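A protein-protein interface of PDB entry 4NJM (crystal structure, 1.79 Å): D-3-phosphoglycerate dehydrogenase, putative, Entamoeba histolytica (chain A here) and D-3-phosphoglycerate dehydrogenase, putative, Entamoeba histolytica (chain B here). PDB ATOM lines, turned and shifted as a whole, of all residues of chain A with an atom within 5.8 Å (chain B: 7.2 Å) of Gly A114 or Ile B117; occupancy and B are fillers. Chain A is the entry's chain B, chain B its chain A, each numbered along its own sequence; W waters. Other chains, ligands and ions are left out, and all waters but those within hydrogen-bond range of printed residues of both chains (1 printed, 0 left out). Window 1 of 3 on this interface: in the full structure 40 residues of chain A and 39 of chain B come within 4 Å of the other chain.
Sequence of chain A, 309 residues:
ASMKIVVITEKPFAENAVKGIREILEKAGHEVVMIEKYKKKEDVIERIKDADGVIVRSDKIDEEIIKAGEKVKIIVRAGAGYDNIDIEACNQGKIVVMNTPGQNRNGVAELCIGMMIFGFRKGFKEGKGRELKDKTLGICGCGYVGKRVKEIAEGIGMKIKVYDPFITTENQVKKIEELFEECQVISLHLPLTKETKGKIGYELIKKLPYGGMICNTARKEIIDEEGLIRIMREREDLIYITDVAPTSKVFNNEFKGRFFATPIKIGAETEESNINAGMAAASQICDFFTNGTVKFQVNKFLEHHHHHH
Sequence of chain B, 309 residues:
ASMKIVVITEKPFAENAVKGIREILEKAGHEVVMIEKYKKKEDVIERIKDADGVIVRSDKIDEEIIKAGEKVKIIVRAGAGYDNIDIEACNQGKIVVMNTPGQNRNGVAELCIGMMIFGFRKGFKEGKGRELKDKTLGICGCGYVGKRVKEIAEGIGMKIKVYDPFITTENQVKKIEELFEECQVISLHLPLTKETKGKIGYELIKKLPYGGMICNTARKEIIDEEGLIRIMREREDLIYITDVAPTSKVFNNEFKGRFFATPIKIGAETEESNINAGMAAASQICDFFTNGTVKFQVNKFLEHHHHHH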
ATOM      1  N   ALA A 109     -10.726 -30.079 -17.748  1.00  0.00           N
ATOM      2  CA  ALA A 109      -9.514 -30.169 -18.568  1.00  0.00           C
ATOM      3  C   ALA A 109      -9.044 -28.813 -19.116  1.00  0.00           C
ATOM      4  O   ALA A 109      -7.846 -28.527 -19.107  1.00  0.00           O
ATOM      5  CB  ALA A 109      -9.696 -31.173 -19.704  1.00  0.00           C
ATOM      6  N   GLU A 110      -9.971 -27.980 -19.595  1.00  0.00           N
ATOM      7  CA  GLU A 110      -9.592 -26.649 -20.082  1.00  0.00           C
ATOM      8  C   GLU A 110      -9.047 -25.774 -18.948  1.00  0.00           C
ATOM      9  O   GLU A 110      -8.042 -25.072 -19.123  1.00  0.00           O
ATOM     10  CB  GLU A 110     -10.754 -25.961 -20.818  1.00  0.00           C
ATOM     11  CG  GLU A 110     -11.009 -26.548 -22.208  1.00  0.00           C
ATOM     12  CD  GLU A 110     -11.917 -25.694 -23.075  1.00  0.00           C
ATOM     13  OE1 GLU A 110     -12.045 -24.476 -22.824  1.00  0.00           O
ATOM     14  OE2 GLU A 110     -12.502 -26.245 -24.022  1.00  0.00           O
ATOM     15  N   LEU A 111      -9.692 -25.835 -17.786  1.00  0.00           N
ATOM     16  CA  LEU A 111      -9.194 -25.110 -16.613  1.00  0.00           C
ATOM     17  C   LEU A 111      -7.786 -25.569 -16.253  1.00  0.00           C
ATOM     18  O   LEU A 111      -6.925 -24.742 -15.968  1.00  0.00           O
ATOM     19  CB  LEU A 111     -10.094 -25.283 -15.387  1.00  0.00           C
ATOM     20  CG  LEU A 111      -9.667 -24.383 -14.216  1.00  0.00           C
ATOM     21  CD1 LEU A 111      -9.826 -22.905 -14.562  1.00  0.00           C
ATOM     22  CD2 LEU A 111     -10.452 -24.716 -12.953  1.00  0.00           C
ATOM     23  N   CYS A 112      -7.576 -26.888 -16.256  1.00  0.00           N
ATOM     24  CA  CYS A 112      -6.277 -27.468 -15.908  1.00  0.00           C
ATOM     25  C   CYS A 112      -5.165 -26.904 -16.796  1.00  0.00           C
ATOM     26  O   CYS A 112      -4.106 -26.498 -16.310  1.00  0.00           O
ATOM     27  CB  CYS A 112      -6.336 -29.001 -16.020  1.00  0.00           C
ATOM     28  SG  CYS A 112      -4.781 -29.816 -15.590  1.00  0.00           S
ATOM     29  N   ILE A 113      -5.403 -26.878 -18.103  1.00  0.00           N
ATOM     30  CA  ILE A 113      -4.406 -26.377 -19.050  1.00  0.00           C
ATOM     31  C   ILE A 113      -4.186 -24.873 -18.851  1.00  0.00           C
ATOM     32  O   ILE A 113      -3.047 -24.396 -18.838  1.00  0.00           O
ATOM     33  CB  ILE A 113      -4.817 -26.699 -20.502  1.00  0.00           C
ATOM     34  CG1 ILE A 113      -4.837 -28.223 -20.731  1.00  0.00           C
ATOM     35  CG2 ILE A 113      -3.911 -25.999 -21.524  1.00  0.00           C
ATOM     36  CD1 ILE A 113      -3.470 -28.895 -20.813  1.00  0.00           C
ATOM     37  N   GLY A 114      -5.279 -24.148 -18.650  1.00  0.00           N
ATOM     38  CA  GLY A 114      -5.222 -22.705 -18.383  1.00  0.00           C
ATOM     39  C   GLY A 114      -4.401 -22.372 -17.149  1.00  0.00           C
ATOM     40  O   GLY A 114      -3.604 -21.437 -17.163  1.00  0.00           O
ATOM     41  N   MET A 115      -4.601 -23.143 -16.078  1.00  0.00           N
ATOM     42  CA  MET A 115      -3.833 -22.981 -14.857  1.00  0.00           C
ATOM     43  C   MET A 115      -2.364 -23.330 -15.061  1.00  0.00           C
ATOM     44  O   MET A 115      -1.506 -22.696 -14.466  1.00  0.00           O
ATOM     45  CB  MET A 115      -4.416 -23.825 -13.717  1.00  0.00           C
ATOM     46  CG  MET A 115      -5.711 -23.276 -13.166  1.00  0.00           C
ATOM     47  SD  MET A 115      -6.403 -24.272 -11.826  1.00  0.00           S
ATOM     48  CE  MET A 115      -7.485 -23.021 -11.166  1.00  0.00           C
ATOM     49  N   MET A 116      -2.068 -24.352 -15.870  1.00  0.00           N
ATOM     50  CA  MET A 116      -0.661 -24.693 -16.116  1.00  0.00           C
ATOM     51  C   MET A 116       0.063 -23.536 -16.814  1.00  0.00           C
ATOM     52  O   MET A 116       1.203 -23.198 -16.460  1.00  0.00           O
ATOM     53  CB  MET A 116      -0.537 -25.996 -16.914  1.00  0.00           C
ATOM     54  CG  MET A 116      -0.963 -27.234 -16.130  1.00  0.00           C
ATOM     55  SD  MET A 116      -1.300 -28.648 -17.219  1.00  0.00           S
ATOM     56  CE  MET A 116       0.131 -28.614 -18.278  1.00  0.00           C
ATOM     57  N   ILE A 117      -0.609 -22.915 -17.777  1.00  0.00           N
ATOM     58  CA  ILE A 117      -0.020 -21.766 -18.481  1.00  0.00           C
ATOM     59  C   ILE A 117       0.136 -20.587 -17.521  1.00  0.00           C
ATOM     60  O   ILE A 117       1.222 -20.033 -17.400  1.00  0.00           O
ATOM     61  CB  ILE A 117      -0.822 -21.381 -19.740  1.00  0.00           C
ATOM     62  CG1 ILE A 117      -0.829 -22.553 -20.735  1.00  0.00           C
ATOM     63  CG2 ILE A 117      -0.242 -20.122 -20.387  1.00  0.00           C
ATOM     64  CD1 ILE A 117      -1.855 -22.409 -21.854  1.00  0.00           C
ATOM     65  N   PHE A 118      -0.943 -20.253 -16.814  1.00  0.00           N
ATOM     66  CA  PHE A 118      -0.961 -19.174 -15.801  1.00  0.00           C
ATOM     67  C   PHE A 118       0.153 -19.375 -14.773  1.00  0.00           C
ATOM     68  O   PHE A 118       0.901 -18.442 -14.448  1.00  0.00           O
ATOM     69  CB  PHE A 118      -2.339 -19.203 -15.114  1.00  0.00           C
ATOM     70  CG  PHE A 118      -2.620 -18.050 -14.173  1.00  0.00           C
ATOM     71  CD1 PHE A 118      -3.041 -16.820 -14.654  1.00  0.00           C
ATOM     72  CD2 PHE A 118      -2.575 -18.244 -12.795  1.00  0.00           C
ATOM     73  CE1 PHE A 118      -3.350 -15.784 -13.780  1.00  0.00           C
ATOM     74  CE2 PHE A 118      -2.878 -17.211 -11.914  1.00  0.00           C
ATOM     75  CZ  PHE A 118      -3.274 -15.982 -12.410  1.00  0.00           C
ATOM     76  N   GLY A 119       0.272 -20.604 -14.269  1.00  0.00           N
ATOM     77  CA  GLY A 119       1.314 -20.946 -13.309  1.00  0.00           C
ATOM     78  C   GLY A 119       2.724 -20.759 -13.837  1.00  0.00           C
ATOM     79  O   GLY A 119       3.590 -20.245 -13.124  1.00  0.00           O
ATOM     80  N   PHE A 124       0.381 -14.141 -15.037  1.00  0.00           N
ATOM     81  CA  PHE A 124       0.208 -13.020 -15.982  1.00  0.00           C
ATOM     82  C   PHE A 124       0.672 -11.676 -15.415  1.00  0.00           C
ATOM     83  O   PHE A 124       0.179 -10.612 -15.807  1.00  0.00           O
ATOM     84  CB  PHE A 124      -1.228 -12.918 -16.530  1.00  0.00           C
ATOM     85  CG  PHE A 124      -1.705 -14.147 -17.269  1.00  0.00           C
ATOM     86  CD1 PHE A 124      -0.810 -15.092 -17.766  1.00  0.00           C
ATOM     87  CD2 PHE A 124      -3.066 -14.342 -17.487  1.00  0.00           C
ATOM     88  CE1 PHE A 124      -1.262 -16.216 -18.444  1.00  0.00           C
ATOM     89  CE2 PHE A 124      -3.523 -15.462 -18.170  1.00  0.00           C
ATOM     90  CZ  PHE A 124      -2.621 -16.399 -18.641  1.00  0.00           C
ATOM     91  N   LEU B 111       0.901 -18.025 -24.385  1.00  0.00           N
ATOM     92  CA  LEU B 111       0.229 -16.934 -23.683  1.00  0.00           C
ATOM     93  C   LEU B 111      -1.165 -16.644 -24.269  1.00  0.00           C
ATOM     94  O   LEU B 111      -2.144 -16.477 -23.534  1.00  0.00           O
ATOM     95  CB  LEU B 111       1.086 -15.667 -23.689  1.00  0.00           C
ATOM     96  CG  LEU B 111       0.426 -14.577 -22.840  1.00  0.00           C
ATOM     97  CD1 LEU B 111       0.496 -14.926 -21.351  1.00  0.00           C
ATOM     98  CD2 LEU B 111       1.057 -13.228 -23.139  1.00  0.00           C
ATOM     99  N   CYS B 112      -1.243 -16.619 -25.594  1.00  0.00           N
ATOM    100  CA  CYS B 112      -2.497 -16.402 -26.296  1.00  0.00           C
ATOM    101  C   CYS B 112      -3.553 -17.420 -25.852  1.00  0.00           C
ATOM    102  O   CYS B 112      -4.666 -17.045 -25.455  1.00  0.00           O
ATOM    103  CB  CYS B 112      -2.264 -16.485 -27.804  1.00  0.00           C
ATOM    104  SG  CYS B 112      -3.720 -16.058 -28.770  1.00  0.00           S
ATOM    105  N   ILE B 113      -3.192 -18.703 -25.877  1.00  0.00           N
ATOM    106  CA  ILE B 113      -4.134 -19.748 -25.485  1.00  0.00           C
ATOM    107  C   ILE B 113      -4.513 -19.624 -24.010  1.00  0.00           C
ATOM    108  O   ILE B 113      -5.686 -19.735 -23.647  1.00  0.00           O
ATOM    109  CB  ILE B 113      -3.568 -21.157 -25.777  1.00  0.00           C
ATOM    110  CG1 ILE B 113      -3.426 -21.378 -27.298  1.00  0.00           C
ATOM    111  CG2 ILE B 113      -4.391 -22.236 -25.074  1.00  0.00           C
ATOM    112  CD1 ILE B 113      -4.725 -21.546 -28.066  1.00  0.00           C
ATOM    113  N   GLY B 114      -3.504 -19.399 -23.171  1.00  0.00           N
ATOM    114  CA  GLY B 114      -3.722 -19.137 -21.753  1.00  0.00           C
ATOM    115  C   GLY B 114      -4.676 -17.983 -21.484  1.00  0.00           C
ATOM    116  O   GLY B 114      -5.542 -18.085 -20.619  1.00  0.00           O
ATOM    117  N   MET B 115      -4.525 -16.879 -22.220  1.00  0.00           N
ATOM    118  CA  MET B 115      -5.414 -15.728 -22.045  1.00  0.00           C
ATOM    119  C   MET B 115      -6.836 -16.015 -22.503  1.00  0.00           C
ATOM    120  O   MET B 115      -7.788 -15.506 -21.920  1.00  0.00           O
ATOM    121  CB  MET B 115      -4.863 -14.505 -22.775  1.00  0.00           C
ATOM    122  CG  MET B 115      -3.611 -13.954 -22.126  1.00  0.00           C
ATOM    123  SD  MET B 115      -3.080 -12.469 -22.989  1.00  0.00           S
ATOM    124  CE  MET B 115      -2.405 -11.585 -21.601  1.00  0.00           C
ATOM    125  N   MET B 116      -6.977 -16.829 -23.549  1.00  0.00           N
ATOM    126  CA  MET B 116      -8.304 -17.228 -24.016  1.00  0.00           C
ATOM    127  C   MET B 116      -9.037 -18.007 -22.936  1.00  0.00           C
ATOM    128  O   MET B 116     -10.216 -17.766 -22.679  1.00  0.00           O
ATOM    129  CB  MET B 116      -8.222 -18.051 -25.309  1.00  0.00           C
ATOM    130  CG  MET B 116      -7.854 -17.240 -26.536  1.00  0.00           C
ATOM    131  SD  MET B 116      -7.535 -18.322 -27.944  1.00  0.00           S
ATOM    132  CE  MET B 116      -7.181 -17.095 -29.183  1.00  0.00           C
ATOM    133  N   ILE B 117      -8.338 -18.945 -22.303  1.00  0.00           N
ATOM    134  CA  ILE B 117      -8.951 -19.738 -21.245  1.00  0.00           C
ATOM    135  C   ILE B 117      -9.312 -18.834 -20.057  1.00  0.00           C
ATOM    136  O   ILE B 117     -10.447 -18.823 -19.600  1.00  0.00           O
ATOM    137  CB  ILE B 117      -8.059 -20.938 -20.818  1.00  0.00           C
ATOM    138  CG1 ILE B 117      -7.816 -21.886 -22.011  1.00  0.00           C
ATOM    139  CG2 ILE B 117      -8.718 -21.679 -19.657  1.00  0.00           C
ATOM    140  CD1 ILE B 117      -6.759 -22.960 -21.763  1.00  0.00           C
ATOM    141  N   PHE B 118      -8.326 -18.076 -19.579  1.00  0.00           N
ATOM    142  CA  PHE B 118      -8.495 -17.091 -18.508  1.00  0.00           C
ATOM    143  C   PHE B 118      -9.689 -16.164 -18.777  1.00  0.00           C
ATOM    144  O   PHE B 118     -10.533 -15.971 -17.900  1.00  0.00           O
ATOM    145  CB  PHE B 118      -7.204 -16.280 -18.422  1.00  0.00           C
ATOM    146  CG  PHE B 118      -7.083 -15.398 -17.208  1.00  0.00           C
ATOM    147  CD1 PHE B 118      -6.785 -15.935 -15.959  1.00  0.00           C
ATOM    148  CD2 PHE B 118      -7.184 -14.022 -17.338  1.00  0.00           C
ATOM    149  CE1 PHE B 118      -6.625 -15.119 -14.855  1.00  0.00           C
ATOM    150  CE2 PHE B 118      -7.020 -13.197 -16.233  1.00  0.00           C
ATOM    151  CZ  PHE B 118      -6.745 -13.745 -14.994  1.00  0.00           C
ATOM    152  N   GLY B 119      -9.747 -15.614 -19.990  1.00  0.00           N
ATOM    153  CA  GLY B 119     -10.830 -14.712 -20.411  1.00  0.00           C
ATOM    154  C   GLY B 119     -12.210 -15.355 -20.386  1.00  0.00           C
ATOM    155  O   GLY B 119     -13.187 -14.719 -19.994  1.00  0.00           O
ATOM    156  N   PHE B 120     -12.286 -16.624 -20.783  1.00  0.00           N
ATOM    157  CA  PHE B 120     -13.552 -17.366 -20.825  1.00  0.00           C
ATOM    158  C   PHE B 120     -13.948 -17.900 -19.449  1.00  0.00           C
ATOM    159  O   PHE B 120     -15.092 -18.312 -19.250  1.00  0.00           O
ATOM    160  CB  PHE B 120     -13.434 -18.540 -21.818  1.00  0.00           C
ATOM    161  CG  PHE B 120     -14.260 -18.393 -23.076  1.00  0.00           C
ATOM    162  CD1 PHE B 120     -14.629 -17.144 -23.569  1.00  0.00           C
ATOM    163  CD2 PHE B 120     -14.634 -19.527 -23.794  1.00  0.00           C
ATOM    164  CE1 PHE B 120     -15.371 -17.032 -24.741  1.00  0.00           C
ATOM    165  CE2 PHE B 120     -15.378 -19.422 -24.964  1.00  0.00           C
ATOM    166  CZ  PHE B 120     -15.747 -18.170 -25.437  1.00  0.00           C
ATOM    167  N   ARG B 121     -13.003 -17.891 -18.508  1.00  0.00           N
ATOM    168  CA  ARG B 121     -13.228 -18.462 -17.174  1.00  0.00           C
ATOM    169  C   ARG B 121     -13.135 -17.411 -16.061  1.00  0.00           C
ATOM    170  O   ARG B 121     -12.605 -17.676 -14.977  1.00  0.00           O
ATOM    171  CB  ARG B 121     -12.267 -19.637 -16.918  1.00  0.00           C
ATOM    172  CG  ARG B 121     -12.395 -20.778 -17.920  1.00  0.00           C
ATOM    173  CD  ARG B 121     -13.766 -21.439 -17.876  1.00  0.00           C
ATOM    174  NE  ARG B 121     -13.905 -22.384 -16.763  1.00  0.00           N
ATOM    175  CZ  ARG B 121     -13.573 -23.675 -16.811  1.00  0.00           C
ATOM    176  NH1 ARG B 121     -13.773 -24.441 -15.743  1.00  0.00           N
ATOM    177  NH2 ARG B 121     -13.056 -24.208 -17.918  1.00  0.00           N
ATOM    178  N   LYS B 122     -13.670 -16.221 -16.350  1.00  0.00           N
ATOM    179  CA  LYS B 122     -13.841 -15.131 -15.368  1.00  0.00           C
ATOM    180  C   LYS B 122     -12.535 -14.710 -14.689  1.00  0.00           C
ATOM    181  O   LYS B 122     -12.533 -14.250 -13.549  1.00  0.00           O
ATOM    182  CB  LYS B 122     -14.893 -15.496 -14.297  1.00  0.00           C
ATOM    183  CG  LYS B 122     -16.198 -16.108 -14.809  1.00  0.00           C
ATOM    184  CD  LYS B 122     -17.039 -15.139 -15.618  1.00  0.00           C
ATOM    185  CE  LYS B 122     -17.883 -14.232 -14.739  1.00  0.00           C
ATOM    186  NZ  LYS B 122     -18.827 -13.477 -15.605  1.00  0.00           N
ATOM    187  N   GLY B 123     -11.416 -14.866 -15.379  1.00  0.00           N
ATOM    188  CA  GLY B 123     -10.127 -14.549 -14.765  1.00  0.00           C
ATOM    189  C   GLY B 123      -9.834 -15.389 -13.533  1.00  0.00           C
ATOM    190  O   GLY B 123      -9.181 -14.921 -12.588  1.00  0.00           O
ATOM    191  N   PHE B 124     -10.327 -16.628 -13.561  1.00  0.00           N
ATOM    192  CA  PHE B 124     -10.213 -17.606 -12.472  1.00  0.00           C
ATOM    193  C   PHE B 124     -10.864 -17.112 -11.184  1.00  0.00           C
ATOM    194  O   PHE B 124     -10.407 -17.426 -10.078  1.00  0.00           O
ATOM    195  CB  PHE B 124      -8.756 -18.071 -12.252  1.00  0.00           C
ATOM    196  CG  PHE B 124      -8.115 -18.692 -13.474  1.00  0.00           C
ATOM    197  CD1 PHE B 124      -8.886 -19.209 -14.513  1.00  0.00           C
ATOM    198  CD2 PHE B 124      -6.727 -18.796 -13.564  1.00  0.00           C
ATOM    199  CE1 PHE B 124      -8.285 -19.786 -15.632  1.00  0.00           C
ATOM    200  CE2 PHE B 124      -6.122 -19.376 -14.677  1.00  0.00           C
ATOM    201  CZ  PHE B 124      -6.901 -19.869 -15.714  1.00  0.00           C
ATOM    202  N   ARG B 130     -17.207 -20.294 -19.748  1.00  0.00           N
ATOM    203  CA  ARG B 130     -17.495 -21.031 -20.971  1.00  0.00           C
ATOM    204  C   ARG B 130     -16.261 -21.795 -21.406  1.00  0.00           C
ATOM    205  O   ARG B 130     -15.166 -21.549 -20.903  1.00  0.00           O
ATOM    206  CB  ARG B 130     -17.909 -20.075 -22.092  1.00  0.00           C
ATOM    207  CG  ARG B 130     -19.222 -19.355 -21.836  1.00  0.00           C
ATOM    208  CD  ARG B 130     -19.617 -18.472 -23.011  1.00  0.00           C
ATOM    209  NE  ARG B 130     -18.694 -17.367 -23.242  1.00  0.00           N
ATOM    210  CZ  ARG B 130     -18.776 -16.172 -22.659  1.00  0.00           C
ATOM    211  NH1 ARG B 130     -19.733 -15.913 -21.775  1.00  0.00           N
ATOM    212  NH2 ARG B 130     -17.888 -15.239 -22.950  1.00  0.00           N
ATOM    213  N   LEU B 132     -13.747 -23.284 -24.616  1.00  0.00           N
ATOM    214  CA  LEU B 132     -13.239 -23.089 -25.976  1.00  0.00           C
ATOM    215  C   LEU B 132     -13.616 -24.216 -26.946  1.00  0.00           C
ATOM    216  O   LEU B 132     -13.835 -23.966 -28.130  1.00  0.00           O
ATOM    217  CB  LEU B 132     -11.719 -22.889 -25.955  1.00  0.00           C
ATOM    218  CG  LEU B 132     -11.233 -21.641 -25.196  1.00  0.00           C
ATOM    219  CD1 LEU B 132      -9.714 -21.651 -25.075  1.00  0.00           C
ATOM    220  CD2 LEU B 132     -11.707 -20.353 -25.860  1.00  0.00           C
ATOM    221  N   ILE B 152      -2.603 -25.592 -31.230  1.00  0.00           N
ATOM    222  CA  ILE B 152      -3.061 -25.772 -29.849  1.00  0.00           C
ATOM    223  C   ILE B 152      -4.583 -25.750 -29.775  1.00  0.00           C
ATOM    224  O   ILE B 152      -5.183 -26.599 -29.119  1.00  0.00           O
ATOM    225  CB  ILE B 152      -2.430 -24.742 -28.896  1.00  0.00           C
ATOM    226  CG1 ILE B 152      -0.895 -24.888 -28.902  1.00  0.00           C
ATOM    227  CG2 ILE B 152      -3.004 -24.906 -27.480  1.00  0.00           C
ATOM    228  CD1 ILE B 152      -0.153 -23.747 -28.226  1.00  0.00           C
ATOM    229  N   ILE B 156      -7.524 -28.403 -28.513  1.00  0.00           N
ATOM    230  CA  ILE B 156      -8.638 -28.019 -27.649  1.00  0.00           C
ATOM    231  C   ILE B 156      -9.974 -28.393 -28.288  1.00  0.00           C
ATOM    232  O   ILE B 156     -10.947 -28.674 -27.589  1.00  0.00           O
ATOM    233  CB  ILE B 156      -8.564 -26.524 -27.264  1.00  0.00           C
ATOM    234  CG1 ILE B 156      -7.360 -26.312 -26.346  1.00  0.00           C
ATOM    235  CG2 ILE B 156      -9.839 -26.060 -26.556  1.00  0.00           C
ATOM    236  CD1 ILE B 156      -7.052 -24.849 -26.048  1.00  0.00           C
ATOM    237  N   MET B 213     -15.256 -12.910 -27.824  1.00  0.00           N
ATOM    238  CA  MET B 213     -14.031 -12.573 -27.101  1.00  0.00           C
ATOM    239  C   MET B 213     -12.935 -12.224 -28.093  1.00  0.00           C
ATOM    240  O   MET B 213     -12.718 -12.951 -29.067  1.00  0.00           O
ATOM    241  CB  MET B 213     -13.576 -13.743 -26.217  1.00  0.00           C
ATOM    242  CG  MET B 213     -12.241 -13.498 -25.517  1.00  0.00           C
ATOM    243  SD  MET B 213     -11.886 -14.718 -24.237  1.00  0.00           S
ATOM    244  CE  MET B 213     -11.743 -16.188 -25.245  1.00  0.00           C
HETATM  245  O   HOH W   1     -12.506 -22.939 -20.493  1.00  0.00           O
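N of Leu B132 is in hydrogen-bond range of OE1 of Glu A110 (2.7 Å).
O of Phe B118 is in hydrogen-bond range of N of Gly B123, 2.9 Å away.
Glu A110 touches Ile B117.
Ile B156 touches Glu A110 (CG2 to OE2, 3.7 Å).
Arg B121 touches Leu A111 (NH2 to N, 3.7 Å).
CD1 of Ile B117 touches N of Gly A114, at 3.6 Å.
Gly A114 touches Phe B124.
Ile A117 touches Gly B114.
Phe A118 touches Phe B124 (CG to CE2, 3.8 Å).
Leu B111 touches Phe A124 (CD1 to CE1, 3.6 Å).
CZ of Phe A124 touches C of Gly B114 (3.8 Å).
Phe B118 touches Phe A124.
Of chain B, only Ile B117 and Phe B124 come within 4 Å of Gly A114.
Of the printed residues of chain A, Leu B132 touches Glu A110 (2.7 Å).
Of the printed residues of chain A, Ile B156 touches Glu A110.
Of the printed residues of chain A, Gly B114 touches Ile A117 and Phe A124.
Of the printed residues of chain A, Arg B121 touches Leu A111 (3.7 Å).
Printed residues of chain B within 4 Å of Ile A117: Gly B114.
Phe B120 touches none of the printed residues of chain A.
Ile B113 touches none of the printed residues of chain A.
The nearest residue of chain B that does not touch Gly A114 is Gly B114 (5.1 Å).
Of the 19 printed residues of chain B, 8 touch a printed residue of chain A.
Of the 12 printed residues of chain A, 6 touch a printed residue of chain B.
Among the printed residues, no Asp or Glu carboxylate lies within 4 Å of a Lys or Arg side-chain nitrogen of the other chain.
Water W1 lies within hydrogen-bond range of the side-chain carboxylate (OE1) of Glu A110, the guanidinium group (NH2) of Arg B121 and the backbone carbonyl oxygen (O) of Arg B130.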
